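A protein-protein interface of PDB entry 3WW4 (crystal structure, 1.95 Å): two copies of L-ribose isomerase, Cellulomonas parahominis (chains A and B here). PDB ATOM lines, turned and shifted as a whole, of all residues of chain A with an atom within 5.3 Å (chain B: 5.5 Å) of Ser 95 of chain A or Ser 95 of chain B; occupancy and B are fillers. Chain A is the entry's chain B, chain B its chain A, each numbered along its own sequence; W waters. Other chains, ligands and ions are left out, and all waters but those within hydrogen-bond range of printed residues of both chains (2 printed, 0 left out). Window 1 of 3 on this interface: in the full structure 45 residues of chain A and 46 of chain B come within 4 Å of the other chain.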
ATOM      1  N   PRO A  79     -14.040  -4.120 -34.195  1.00  0.00           N
ATOM      2  CA  PRO A  79     -13.944  -4.487 -32.780  1.00  0.00           C
ATOM      3  C   PRO A  79     -13.514  -5.940 -32.584  1.00  0.00           C
ATOM      4  O   PRO A  79     -12.752  -6.248 -31.666  1.00  0.00           O
ATOM      5  CB  PRO A  79     -15.359  -4.235 -32.267  1.00  0.00           C
ATOM      6  CG  PRO A  79     -15.844  -3.113 -33.147  1.00  0.00           C
ATOM      7  CD  PRO A  79     -15.375  -3.572 -34.503  1.00  0.00           C
ATOM      8  N   ALA A  80     -14.003  -6.824 -33.453  1.00  0.00           N
ATOM      9  CA  ALA A  80     -13.688  -8.250 -33.371  1.00  0.00           C
ATOM     10  C   ALA A  80     -14.182  -8.772 -32.025  1.00  0.00           C
ATOM     11  O   ALA A  80     -13.534  -9.592 -31.370  1.00  0.00           O
ATOM     12  CB  ALA A  80     -12.177  -8.488 -33.522  1.00  0.00           C
ATOM     13  N   HIS A  91     -11.032  -7.263 -21.498  1.00  0.00           N
ATOM     14  CA  HIS A  91      -9.797  -6.966 -22.206  1.00  0.00           C
ATOM     15  C   HIS A  91      -9.956  -6.930 -23.719  1.00  0.00           C
ATOM     16  O   HIS A  91      -8.975  -6.854 -24.458  1.00  0.00           O
ATOM     17  CB  HIS A  91      -8.735  -7.974 -21.777  1.00  0.00           C
ATOM     18  CG  HIS A  91      -8.446  -7.926 -20.308  1.00  0.00           C
ATOM     19  ND1 HIS A  91      -7.675  -6.936 -19.735  1.00  0.00           N
ATOM     20  CD2 HIS A  91      -8.910  -8.682 -19.284  1.00  0.00           C
ATOM     21  CE1 HIS A  91      -7.677  -7.082 -18.422  1.00  0.00           C
ATOM     22  NE2 HIS A  91      -8.420  -8.133 -18.122  1.00  0.00           N
ATOM     23  N   ALA A  92     -11.205  -6.959 -24.170  1.00  0.00           N
ATOM     24  CA  ALA A  92     -11.514  -6.916 -25.591  1.00  0.00           C
ATOM     25  C   ALA A  92     -11.012  -5.607 -26.210  1.00  0.00           C
ATOM     26  O   ALA A  92     -10.612  -5.560 -27.377  1.00  0.00           O
ATOM     27  CB  ALA A  92     -13.020  -7.039 -25.789  1.00  0.00           C
ATOM     28  N   GLU A  93     -11.031  -4.550 -25.408  1.00  0.00           N
ATOM     29  CA  GLU A  93     -10.614  -3.231 -25.856  1.00  0.00           C
ATOM     30  C   GLU A  93      -9.154  -3.179 -26.283  1.00  0.00           C
ATOM     31  O   GLU A  93      -8.739  -2.228 -26.943  1.00  0.00           O
ATOM     32  CB  GLU A  93     -10.885  -2.196 -24.755  1.00  0.00           C
ATOM     33  CG  GLU A  93     -10.140  -2.449 -23.445  1.00  0.00           C
ATOM     34  CD  GLU A  93     -10.739  -1.681 -22.279  1.00  0.00           C
ATOM     35  OE1 GLU A  93     -11.912  -1.947 -21.938  1.00  0.00           O
ATOM     36  OE2 GLU A  93     -10.049  -0.811 -21.705  1.00  0.00           O
ATOM     37  N   TYR A  94      -8.377  -4.194 -25.900  1.00  0.00           N
ATOM     38  CA  TYR A  94      -6.963  -4.258 -26.269  1.00  0.00           C
ATOM     39  C   TYR A  94      -6.813  -5.031 -27.576  1.00  0.00           C
ATOM     40  O   TYR A  94      -5.712  -5.148 -28.118  1.00  0.00           O
ATOM     41  CB  TYR A  94      -6.143  -4.969 -25.185  1.00  0.00           C
ATOM     42  CG  TYR A  94      -6.047  -4.215 -23.881  1.00  0.00           C
ATOM     43  CD1 TYR A  94      -7.123  -4.173 -22.989  1.00  0.00           C
ATOM     44  CD2 TYR A  94      -4.893  -3.503 -23.557  1.00  0.00           C
ATOM     45  CE1 TYR A  94      -7.048  -3.437 -21.806  1.00  0.00           C
ATOM     46  CE2 TYR A  94      -4.809  -2.771 -22.389  1.00  0.00           C
ATOM     47  CZ  TYR A  94      -5.887  -2.736 -21.516  1.00  0.00           C
ATOM     48  OH  TYR A  94      -5.792  -1.992 -20.362  1.00  0.00           O
ATOM     49  N   SER A  95      -7.927  -5.564 -28.070  1.00  0.00           N
ATOM     50  CA  SER A  95      -7.923  -6.342 -29.297  1.00  0.00           C
ATOM     51  C   SER A  95      -8.560  -5.574 -30.462  1.00  0.00           C
ATOM     52  O   SER A  95      -8.526  -4.346 -30.497  1.00  0.00           O
ATOM     53  CB  SER A  95      -8.659  -7.659 -29.062  1.00  0.00           C
ATOM     54  OG  SER A  95      -8.486  -8.544 -30.155  1.00  0.00           O
ATOM     55  N   GLY A  96      -9.146  -6.298 -31.409  1.00  0.00           N
ATOM     56  CA  GLY A  96      -9.762  -5.649 -32.553  1.00  0.00           C
ATOM     57  C   GLY A  96      -8.774  -5.490 -33.699  1.00  0.00           C
ATOM     58  O   GLY A  96      -7.579  -5.738 -33.537  1.00  0.00           O
ATOM     59  N   LEU A  97      -9.277  -5.074 -34.857  1.00  0.00           N
ATOM     60  CA  LEU A  97      -8.450  -4.879 -36.045  1.00  0.00           C
ATOM     61  C   LEU A  97      -8.683  -3.510 -36.671  1.00  0.00           C
ATOM     62  O   LEU A  97      -9.822  -3.099 -36.890  1.00  0.00           O
ATOM     63  CB  LEU A  97      -8.755  -5.962 -37.088  1.00  0.00           C
ATOM     64  CG  LEU A  97      -8.443  -7.395 -36.658  1.00  0.00           C
ATOM     65  CD1 LEU A  97      -9.003  -8.393 -37.680  1.00  0.00           C
ATOM     66  CD2 LEU A  97      -6.945  -7.537 -36.490  1.00  0.00           C
ATOM     67  N   ARG A 191       1.763  -1.223 -27.421  1.00  0.00           N
ATOM     68  CA  ARG A 191       0.968  -0.306 -26.620  1.00  0.00           C
ATOM     69  C   ARG A 191       1.796   0.152 -25.411  1.00  0.00           C
ATOM     70  O   ARG A 191       2.746  -0.527 -25.000  1.00  0.00           O
ATOM     71  CB  ARG A 191      -0.295  -1.020 -26.135  1.00  0.00           C
ATOM     72  CG  ARG A 191       0.004  -2.316 -25.388  1.00  0.00           C
ATOM     73  CD  ARG A 191      -1.247  -2.898 -24.746  1.00  0.00           C
ATOM     74  NE  ARG A 191      -2.135  -3.545 -25.704  1.00  0.00           N
ATOM     75  CZ  ARG A 191      -1.948  -4.765 -26.205  1.00  0.00           C
ATOM     76  NH1 ARG A 191      -0.894  -5.489 -25.845  1.00  0.00           N
ATOM     77  NH2 ARG A 191      -2.831  -5.272 -27.054  1.00  0.00           N
ATOM     78  N   THR A 214      -4.536  -2.761 -33.474  1.00  0.00           N
ATOM     79  CA  THR A 214      -5.714  -3.261 -32.797  1.00  0.00           C
ATOM     80  C   THR A 214      -6.691  -2.087 -32.849  1.00  0.00           C
ATOM     81  O   THR A 214      -6.320  -1.000 -33.290  1.00  0.00           O
ATOM     82  CB  THR A 214      -5.408  -3.656 -31.347  1.00  0.00           C
ATOM     83  OG1 THR A 214      -4.836  -2.541 -30.654  1.00  0.00           O
ATOM     84  CG2 THR A 214      -4.437  -4.840 -31.318  1.00  0.00           C
ATOM     85  N   TYR A 215      -7.927  -2.299 -32.414  1.00  0.00           N
ATOM     86  CA  TYR A 215      -8.950  -1.253 -32.462  1.00  0.00           C
ATOM     87  C   TYR A 215      -8.501   0.155 -32.051  1.00  0.00           C
ATOM     88  O   TYR A 215      -7.803   0.324 -31.047  1.00  0.00           O
ATOM     89  CB  TYR A 215     -10.138  -1.656 -31.592  1.00  0.00           C
ATOM     90  CG  TYR A 215     -11.404  -0.903 -31.907  1.00  0.00           C
ATOM     91  CD1 TYR A 215     -12.186  -1.250 -33.005  1.00  0.00           C
ATOM     92  CD2 TYR A 215     -11.832   0.151 -31.096  1.00  0.00           C
ATOM     93  CE1 TYR A 215     -13.365  -0.573 -33.287  1.00  0.00           C
ATOM     94  CE2 TYR A 215     -13.010   0.839 -31.369  1.00  0.00           C
ATOM     95  CZ  TYR A 215     -13.774   0.468 -32.464  1.00  0.00           C
ATOM     96  OH  TYR A 215     -14.962   1.117 -32.724  1.00  0.00           O
ATOM     97  N   TRP A 233     -16.791   0.221 -23.874  1.00  0.00           N
ATOM     98  CA  TRP A 233     -16.152   1.002 -24.931  1.00  0.00           C
ATOM     99  C   TRP A 233     -16.772   2.362 -25.182  1.00  0.00           C
ATOM    100  O   TRP A 233     -16.235   3.154 -25.956  1.00  0.00           O
ATOM    101  CB  TRP A 233     -16.169   0.224 -26.244  1.00  0.00           C
ATOM    102  CG  TRP A 233     -15.369  -1.031 -26.230  1.00  0.00           C
ATOM    103  CD1 TRP A 233     -15.124  -1.840 -25.159  1.00  0.00           C
ATOM    104  CD2 TRP A 233     -14.791  -1.680 -27.365  1.00  0.00           C
ATOM    105  NE1 TRP A 233     -14.433  -2.957 -25.558  1.00  0.00           N
ATOM    106  CE2 TRP A 233     -14.217  -2.886 -26.908  1.00  0.00           C
ATOM    107  CE3 TRP A 233     -14.706  -1.359 -28.727  1.00  0.00           C
ATOM    108  CZ2 TRP A 233     -13.566  -3.777 -27.764  1.00  0.00           C
ATOM    109  CZ3 TRP A 233     -14.056  -2.245 -29.581  1.00  0.00           C
ATOM    110  CH2 TRP A 233     -13.494  -3.442 -29.094  1.00  0.00           C
ATOM    111  N   GLU B  78       1.969 -10.884 -35.049  1.00  0.00           N
ATOM    112  CA  GLU B  78       2.309 -10.298 -33.763  1.00  0.00           C
ATOM    113  C   GLU B  78       1.339 -10.725 -32.650  1.00  0.00           C
ATOM    114  O   GLU B  78       0.133 -10.488 -32.735  1.00  0.00           O
ATOM    115  CB  GLU B  78       2.286  -8.771 -33.926  1.00  0.00           C
ATOM    116  CG  GLU B  78       2.363  -7.964 -32.652  1.00  0.00           C
ATOM    117  CD  GLU B  78       3.620  -8.257 -31.857  1.00  0.00           C
ATOM    118  OE1 GLU B  78       4.717  -8.283 -32.460  1.00  0.00           O
ATOM    119  OE2 GLU B  78       3.503  -8.453 -30.631  1.00  0.00           O
ATOM    120  N   PRO B  79       1.857 -11.359 -31.589  1.00  0.00           N
ATOM    121  CA  PRO B  79       1.003 -11.797 -30.483  1.00  0.00           C
ATOM    122  C   PRO B  79       0.294 -10.635 -29.791  1.00  0.00           C
ATOM    123  O   PRO B  79      -0.797 -10.804 -29.236  1.00  0.00           O
ATOM    124  CB  PRO B  79       1.983 -12.507 -29.559  1.00  0.00           C
ATOM    125  CG  PRO B  79       3.008 -13.047 -30.512  1.00  0.00           C
ATOM    126  CD  PRO B  79       3.225 -11.884 -31.429  1.00  0.00           C
ATOM    127  N   ALA B  80       0.921  -9.460 -29.829  1.00  0.00           N
ATOM    128  CA  ALA B  80       0.379  -8.256 -29.200  1.00  0.00           C
ATOM    129  C   ALA B  80       0.083  -8.489 -27.725  1.00  0.00           C
ATOM    130  O   ALA B  80      -0.846  -7.913 -27.162  1.00  0.00           O
ATOM    131  CB  ALA B  80      -0.884  -7.789 -29.924  1.00  0.00           C
ATOM    132  N   HIS B  91      -7.694 -14.793 -22.683  1.00  0.00           N
ATOM    133  CA  HIS B  91      -8.219 -14.576 -24.027  1.00  0.00           C
ATOM    134  C   HIS B  91      -7.316 -13.817 -24.986  1.00  0.00           C
ATOM    135  O   HIS B  91      -7.775 -13.345 -26.024  1.00  0.00           O
ATOM    136  CB  HIS B  91      -9.570 -13.872 -23.942  1.00  0.00           C
ATOM    137  CG  HIS B  91     -10.577 -14.618 -23.131  1.00  0.00           C
ATOM    138  ND1 HIS B  91     -10.594 -14.584 -21.752  1.00  0.00           N
ATOM    139  CD2 HIS B  91     -11.559 -15.474 -23.500  1.00  0.00           C
ATOM    140  CE1 HIS B  91     -11.544 -15.387 -21.308  1.00  0.00           C
ATOM    141  NE2 HIS B  91     -12.143 -15.940 -22.346  1.00  0.00           N
ATOM    142  N   ALA B  92      -6.035 -13.713 -24.656  1.00  0.00           N
ATOM    143  CA  ALA B  92      -5.101 -12.995 -25.515  1.00  0.00           C
ATOM    144  C   ALA B  92      -4.952 -13.699 -26.860  1.00  0.00           C
ATOM    145  O   ALA B  92      -4.597 -13.075 -27.864  1.00  0.00           O
ATOM    146  CB  ALA B  92      -3.740 -12.874 -24.828  1.00  0.00           C
ATOM    147  N   GLU B  93      -5.233 -14.998 -26.871  1.00  0.00           N
ATOM    148  CA  GLU B  93      -5.117 -15.799 -28.088  1.00  0.00           C
ATOM    149  C   GLU B  93      -6.159 -15.402 -29.134  1.00  0.00           C
ATOM    150  O   GLU B  93      -6.063 -15.798 -30.299  1.00  0.00           O
ATOM    151  CB  GLU B  93      -5.263 -17.284 -27.742  1.00  0.00           C
ATOM    152  CG  GLU B  93      -6.632 -17.653 -27.200  1.00  0.00           C
ATOM    153  CD  GLU B  93      -6.612 -18.959 -26.440  1.00  0.00           C
ATOM    154  OE1 GLU B  93      -5.820 -19.060 -25.479  1.00  0.00           O
ATOM    155  OE2 GLU B  93      -7.381 -19.879 -26.800  1.00  0.00           O
ATOM    156  N   TYR B  94      -7.156 -14.628 -28.714  1.00  0.00           N
ATOM    157  CA  TYR B  94      -8.201 -14.172 -29.624  1.00  0.00           C
ATOM    158  C   TYR B  94      -7.817 -12.843 -30.258  1.00  0.00           C
ATOM    159  O   TYR B  94      -8.489 -12.360 -31.162  1.00  0.00           O
ATOM    160  CB  TYR B  94      -9.533 -14.004 -28.890  1.00  0.00           C
ATOM    161  CG  TYR B  94     -10.138 -15.308 -28.451  1.00  0.00           C
ATOM    162  CD1 TYR B  94      -9.688 -15.960 -27.297  1.00  0.00           C
ATOM    163  CD2 TYR B  94     -11.133 -15.922 -29.214  1.00  0.00           C
ATOM    164  CE1 TYR B  94     -10.218 -17.200 -26.918  1.00  0.00           C
ATOM    165  CE2 TYR B  94     -11.668 -17.153 -28.847  1.00  0.00           C
ATOM    166  CZ  TYR B  94     -11.206 -17.787 -27.702  1.00  0.00           C
ATOM    167  OH  TYR B  94     -11.727 -19.014 -27.363  1.00  0.00           O
ATOM    168  N   SER B  95      -6.729 -12.260 -29.775  1.00  0.00           N
ATOM    169  CA  SER B  95      -6.276 -10.983 -30.291  1.00  0.00           C
ATOM    170  C   SER B  95      -5.048 -11.167 -31.181  1.00  0.00           C
ATOM    171  O   SER B  95      -4.954 -12.144 -31.919  1.00  0.00           O
ATOM    172  CB  SER B  95      -5.968 -10.045 -29.127  1.00  0.00           C
ATOM    173  OG  SER B  95      -5.632  -8.749 -29.589  1.00  0.00           O
ATOM    174  N   GLY B  96      -4.108 -10.236 -31.104  1.00  0.00           N
ATOM    175  CA  GLY B  96      -2.925 -10.332 -31.931  1.00  0.00           C
ATOM    176  C   GLY B  96      -3.172  -9.654 -33.269  1.00  0.00           C
ATOM    177  O   GLY B  96      -4.292  -9.233 -33.555  1.00  0.00           O
ATOM    178  N   LEU B  97      -2.118  -9.558 -34.081  1.00  0.00           N
ATOM    179  CA  LEU B  97      -2.174  -8.927 -35.399  1.00  0.00           C
ATOM    180  C   LEU B  97      -1.480  -9.794 -36.437  1.00  0.00           C
ATOM    181  O   LEU B  97      -0.336 -10.201 -36.255  1.00  0.00           O
ATOM    182  CB  LEU B  97      -1.485  -7.562 -35.359  1.00  0.00           C
ATOM    183  CG  LEU B  97      -2.180  -6.496 -34.514  1.00  0.00           C
ATOM    184  CD1 LEU B  97      -1.320  -5.243 -34.444  1.00  0.00           C
ATOM    185  CD2 LEU B  97      -3.542  -6.184 -35.115  1.00  0.00           C
ATOM    186  N   ARG B 191     -14.646 -14.718 -36.537  1.00  0.00           N
ATOM    187  CA  ARG B 191     -14.194 -16.010 -36.048  1.00  0.00           C
ATOM    188  C   ARG B 191     -15.423 -16.895 -35.837  1.00  0.00           C
ATOM    189  O   ARG B 191     -16.520 -16.392 -35.583  1.00  0.00           O
ATOM    190  CB  ARG B 191     -13.456 -15.835 -34.716  1.00  0.00           C
ATOM    191  CG  ARG B 191     -14.318 -15.213 -33.612  1.00  0.00           C
ATOM    192  CD  ARG B 191     -13.581 -15.179 -32.288  1.00  0.00           C
ATOM    193  NE  ARG B 191     -12.456 -14.250 -32.295  1.00  0.00           N
ATOM    194  CZ  ARG B 191     -12.552 -12.962 -31.976  1.00  0.00           C
ATOM    195  NH1 ARG B 191     -13.728 -12.450 -31.621  1.00  0.00           N
ATOM    196  NH2 ARG B 191     -11.475 -12.186 -32.003  1.00  0.00           N
ATOM    197  N   THR B 214      -6.431 -11.262 -36.704  1.00  0.00           N
ATOM    198  CA  THR B 214      -5.890 -11.455 -35.372  1.00  0.00           C
ATOM    199  C   THR B 214      -4.830 -12.545 -35.512  1.00  0.00           C
ATOM    200  O   THR B 214      -4.666 -13.111 -36.596  1.00  0.00           O
ATOM    201  CB  THR B 214      -7.000 -11.887 -34.374  1.00  0.00           C
ATOM    202  OG1 THR B 214      -7.679 -13.048 -34.870  1.00  0.00           O
ATOM    203  CG2 THR B 214      -8.011 -10.757 -34.190  1.00  0.00           C
ATOM    204  N   TYR B 215      -4.126 -12.846 -34.425  1.00  0.00           N
ATOM    205  CA  TYR B 215      -3.054 -13.841 -34.445  1.00  0.00           C
ATOM    206  C   TYR B 215      -3.406 -15.164 -35.113  1.00  0.00           C
ATOM    207  O   TYR B 215      -4.467 -15.744 -34.883  1.00  0.00           O
ATOM    208  CB  TYR B 215      -2.552 -14.121 -33.030  1.00  0.00           C
ATOM    209  CG  TYR B 215      -1.227 -14.851 -33.007  1.00  0.00           C
ATOM    210  CD1 TYR B 215      -0.033 -14.168 -33.223  1.00  0.00           C
ATOM    211  CD2 TYR B 215      -1.171 -16.224 -32.771  1.00  0.00           C
ATOM    212  CE1 TYR B 215       1.187 -14.834 -33.200  1.00  0.00           C
ATOM    213  CE2 TYR B 215       0.036 -16.897 -32.743  1.00  0.00           C
ATOM    214  CZ  TYR B 215       1.216 -16.197 -32.958  1.00  0.00           C
ATOM    215  OH  TYR B 215       2.416 -16.870 -32.921  1.00  0.00           O
HETATM  216  O   HOH W   1      -6.466  -7.946 -32.194  1.00  0.00           O
HETATM  217  O   HOH W   2      -4.113  -7.973 -27.176  1.00  0.00           O
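The backbone carbonyl oxygen (O) of Ala 80 of chain B is in hydrogen-bond range of the guanidinium group (NH1) of Arg 191 of chain A, 2.8 Å away. The side-chain hydroxyl (OG) of Ser 95 of chain B sits at hydrogen-bond distance from the side-chain hydroxyl (OG) of Ser 95 of chain A (2.9 Å). NH1 of Arg 191 of chain B sits at hydrogen-bond distance from O of Ala 80 of chain A, at 2.9 Å.
O of Ser 95 of chain A is in hydrogen-bond range of N of Tyr 215 of chain A, 2.9 Å away. The backbone NH (N) of Tyr 215 of chain B is in hydrogen-bond range of the backbone carbonyl oxygen (O) of Ser 95 of chain B (2.7 Å). The backbone NH (N) of Ala 80 of chain B lies within hydrogen-bond range of the side-chain carboxylate (OE2) of Glu 78 of chain B (2.9 Å). The backbone carbonyl oxygen (O) of Leu 97 of chain B sits at hydrogen-bond distance from the backbone NH (N) of Glu 78 of chain B (2.7 Å). The backbone carbonyl oxygen (O) of Tyr 94 of chain B sits at hydrogen-bond distance from the guanidinium group (NH2) of Arg 191 of chain B. The backbone carbonyl oxygen of Tyr 94 of chain A lies within hydrogen-bond range of the guanidinium group of Arg 191 of chain A (3.1 Å).
Tyr 94 of chain A touches Ser 95 of chain B (O to OG, 3.9 Å). Ser 95 of chain A touches Tyr 94 of chain B. CD2 of Leu 97 of chain A touches CD2 of Leu 97 of chain B, 3.9 Å away. Leu 97 of chain A touches Thr 214 of chain B (CD2 to N, 3.8 Å). Leu 97 of chain B touches Thr 214 of chain A.
Printed residues of chain B within 4 Å of Ser 95 of chain A: Tyr 94 (3.9 Å) and Ser 95 (2.9 Å). Trp 233 of chain A touches none of the printed residues of chain B. Of the printed residues of chain A, Ala 80 of chain B touches Arg 191. Of the printed residues of chain A, Tyr 94 of chain B touches Ser 95 (3.9 Å). Of chain A, only Tyr 94 and Ser 95 come within 4 Å of Ser 95 of chain B. Printed residues of chain A within 4 Å of Arg 191 of chain B: Ala 80. Printed residues of chain A within 4 Å of Thr 214 of chain B: Leu 97. The nearest residue of chain A that does not touch Ser 95 of chain B is Thr 214 of chain A (4.4 Å).
Of the 13 printed residues of chain A, 6 touch a printed residue of chain B. Hydrophobic or aromatic side chains of chain A within 4 Å of the printed part of chain B: Leu 97. Along chain A the printed residues that touch a printed residue of chain B span positions 80 to 214. Printed residues of chain B that touch a printed residue of chain A: Ala 80, Tyr 94, Ser 95, Leu 97, Arg 191 and Thr 214. Among the printed residues, 8 pairs touch across the chains. Among the printed residues, no Asp or Glu carboxylate lies within 4 Å of a Lys or Arg side-chain nitrogen of the other chain.
Ala 80 of chain A touches Arg 191 of chain B, and with the chains exchanged Arg 191 of chain A touches Ala 80 of chain B. Tyr 94 of chain A touches Ser 95 of chain B, and with the chains exchanged Ser 95 of chain A touches Tyr 94 of chain B. Leu 97 of chain B touches its own counterpart, Leu 97 of chain A. Leu 97 of chain A touches Thr 214 of chain B, and with the chains exchanged Thr 214 of chain A touches Leu 97 of chain B. 12 positions are printed for both chains. Of the 8 pairs that touch across the chains among the printed residues, 8 have their exchanged pair printed and touching as well.
Water W1 lies within hydrogen-bond range of O of Gly 96 of chain A (2.8 Å), OG of Ser 95 of chain B (2.9 Å), O of Gly 96 of chain B (2.9 Å) and OG of Ser 95 of chain A (2.9 Å). Water W2 lies within hydrogen-bond range of OG of Ser 95 of chain B (3.0 Å), NH2 of Arg 191 of chain A (3.0 Å), O of Ala 80 of chain B (3.3 Å) and O of Tyr 94 of chain A (3.4 Å).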
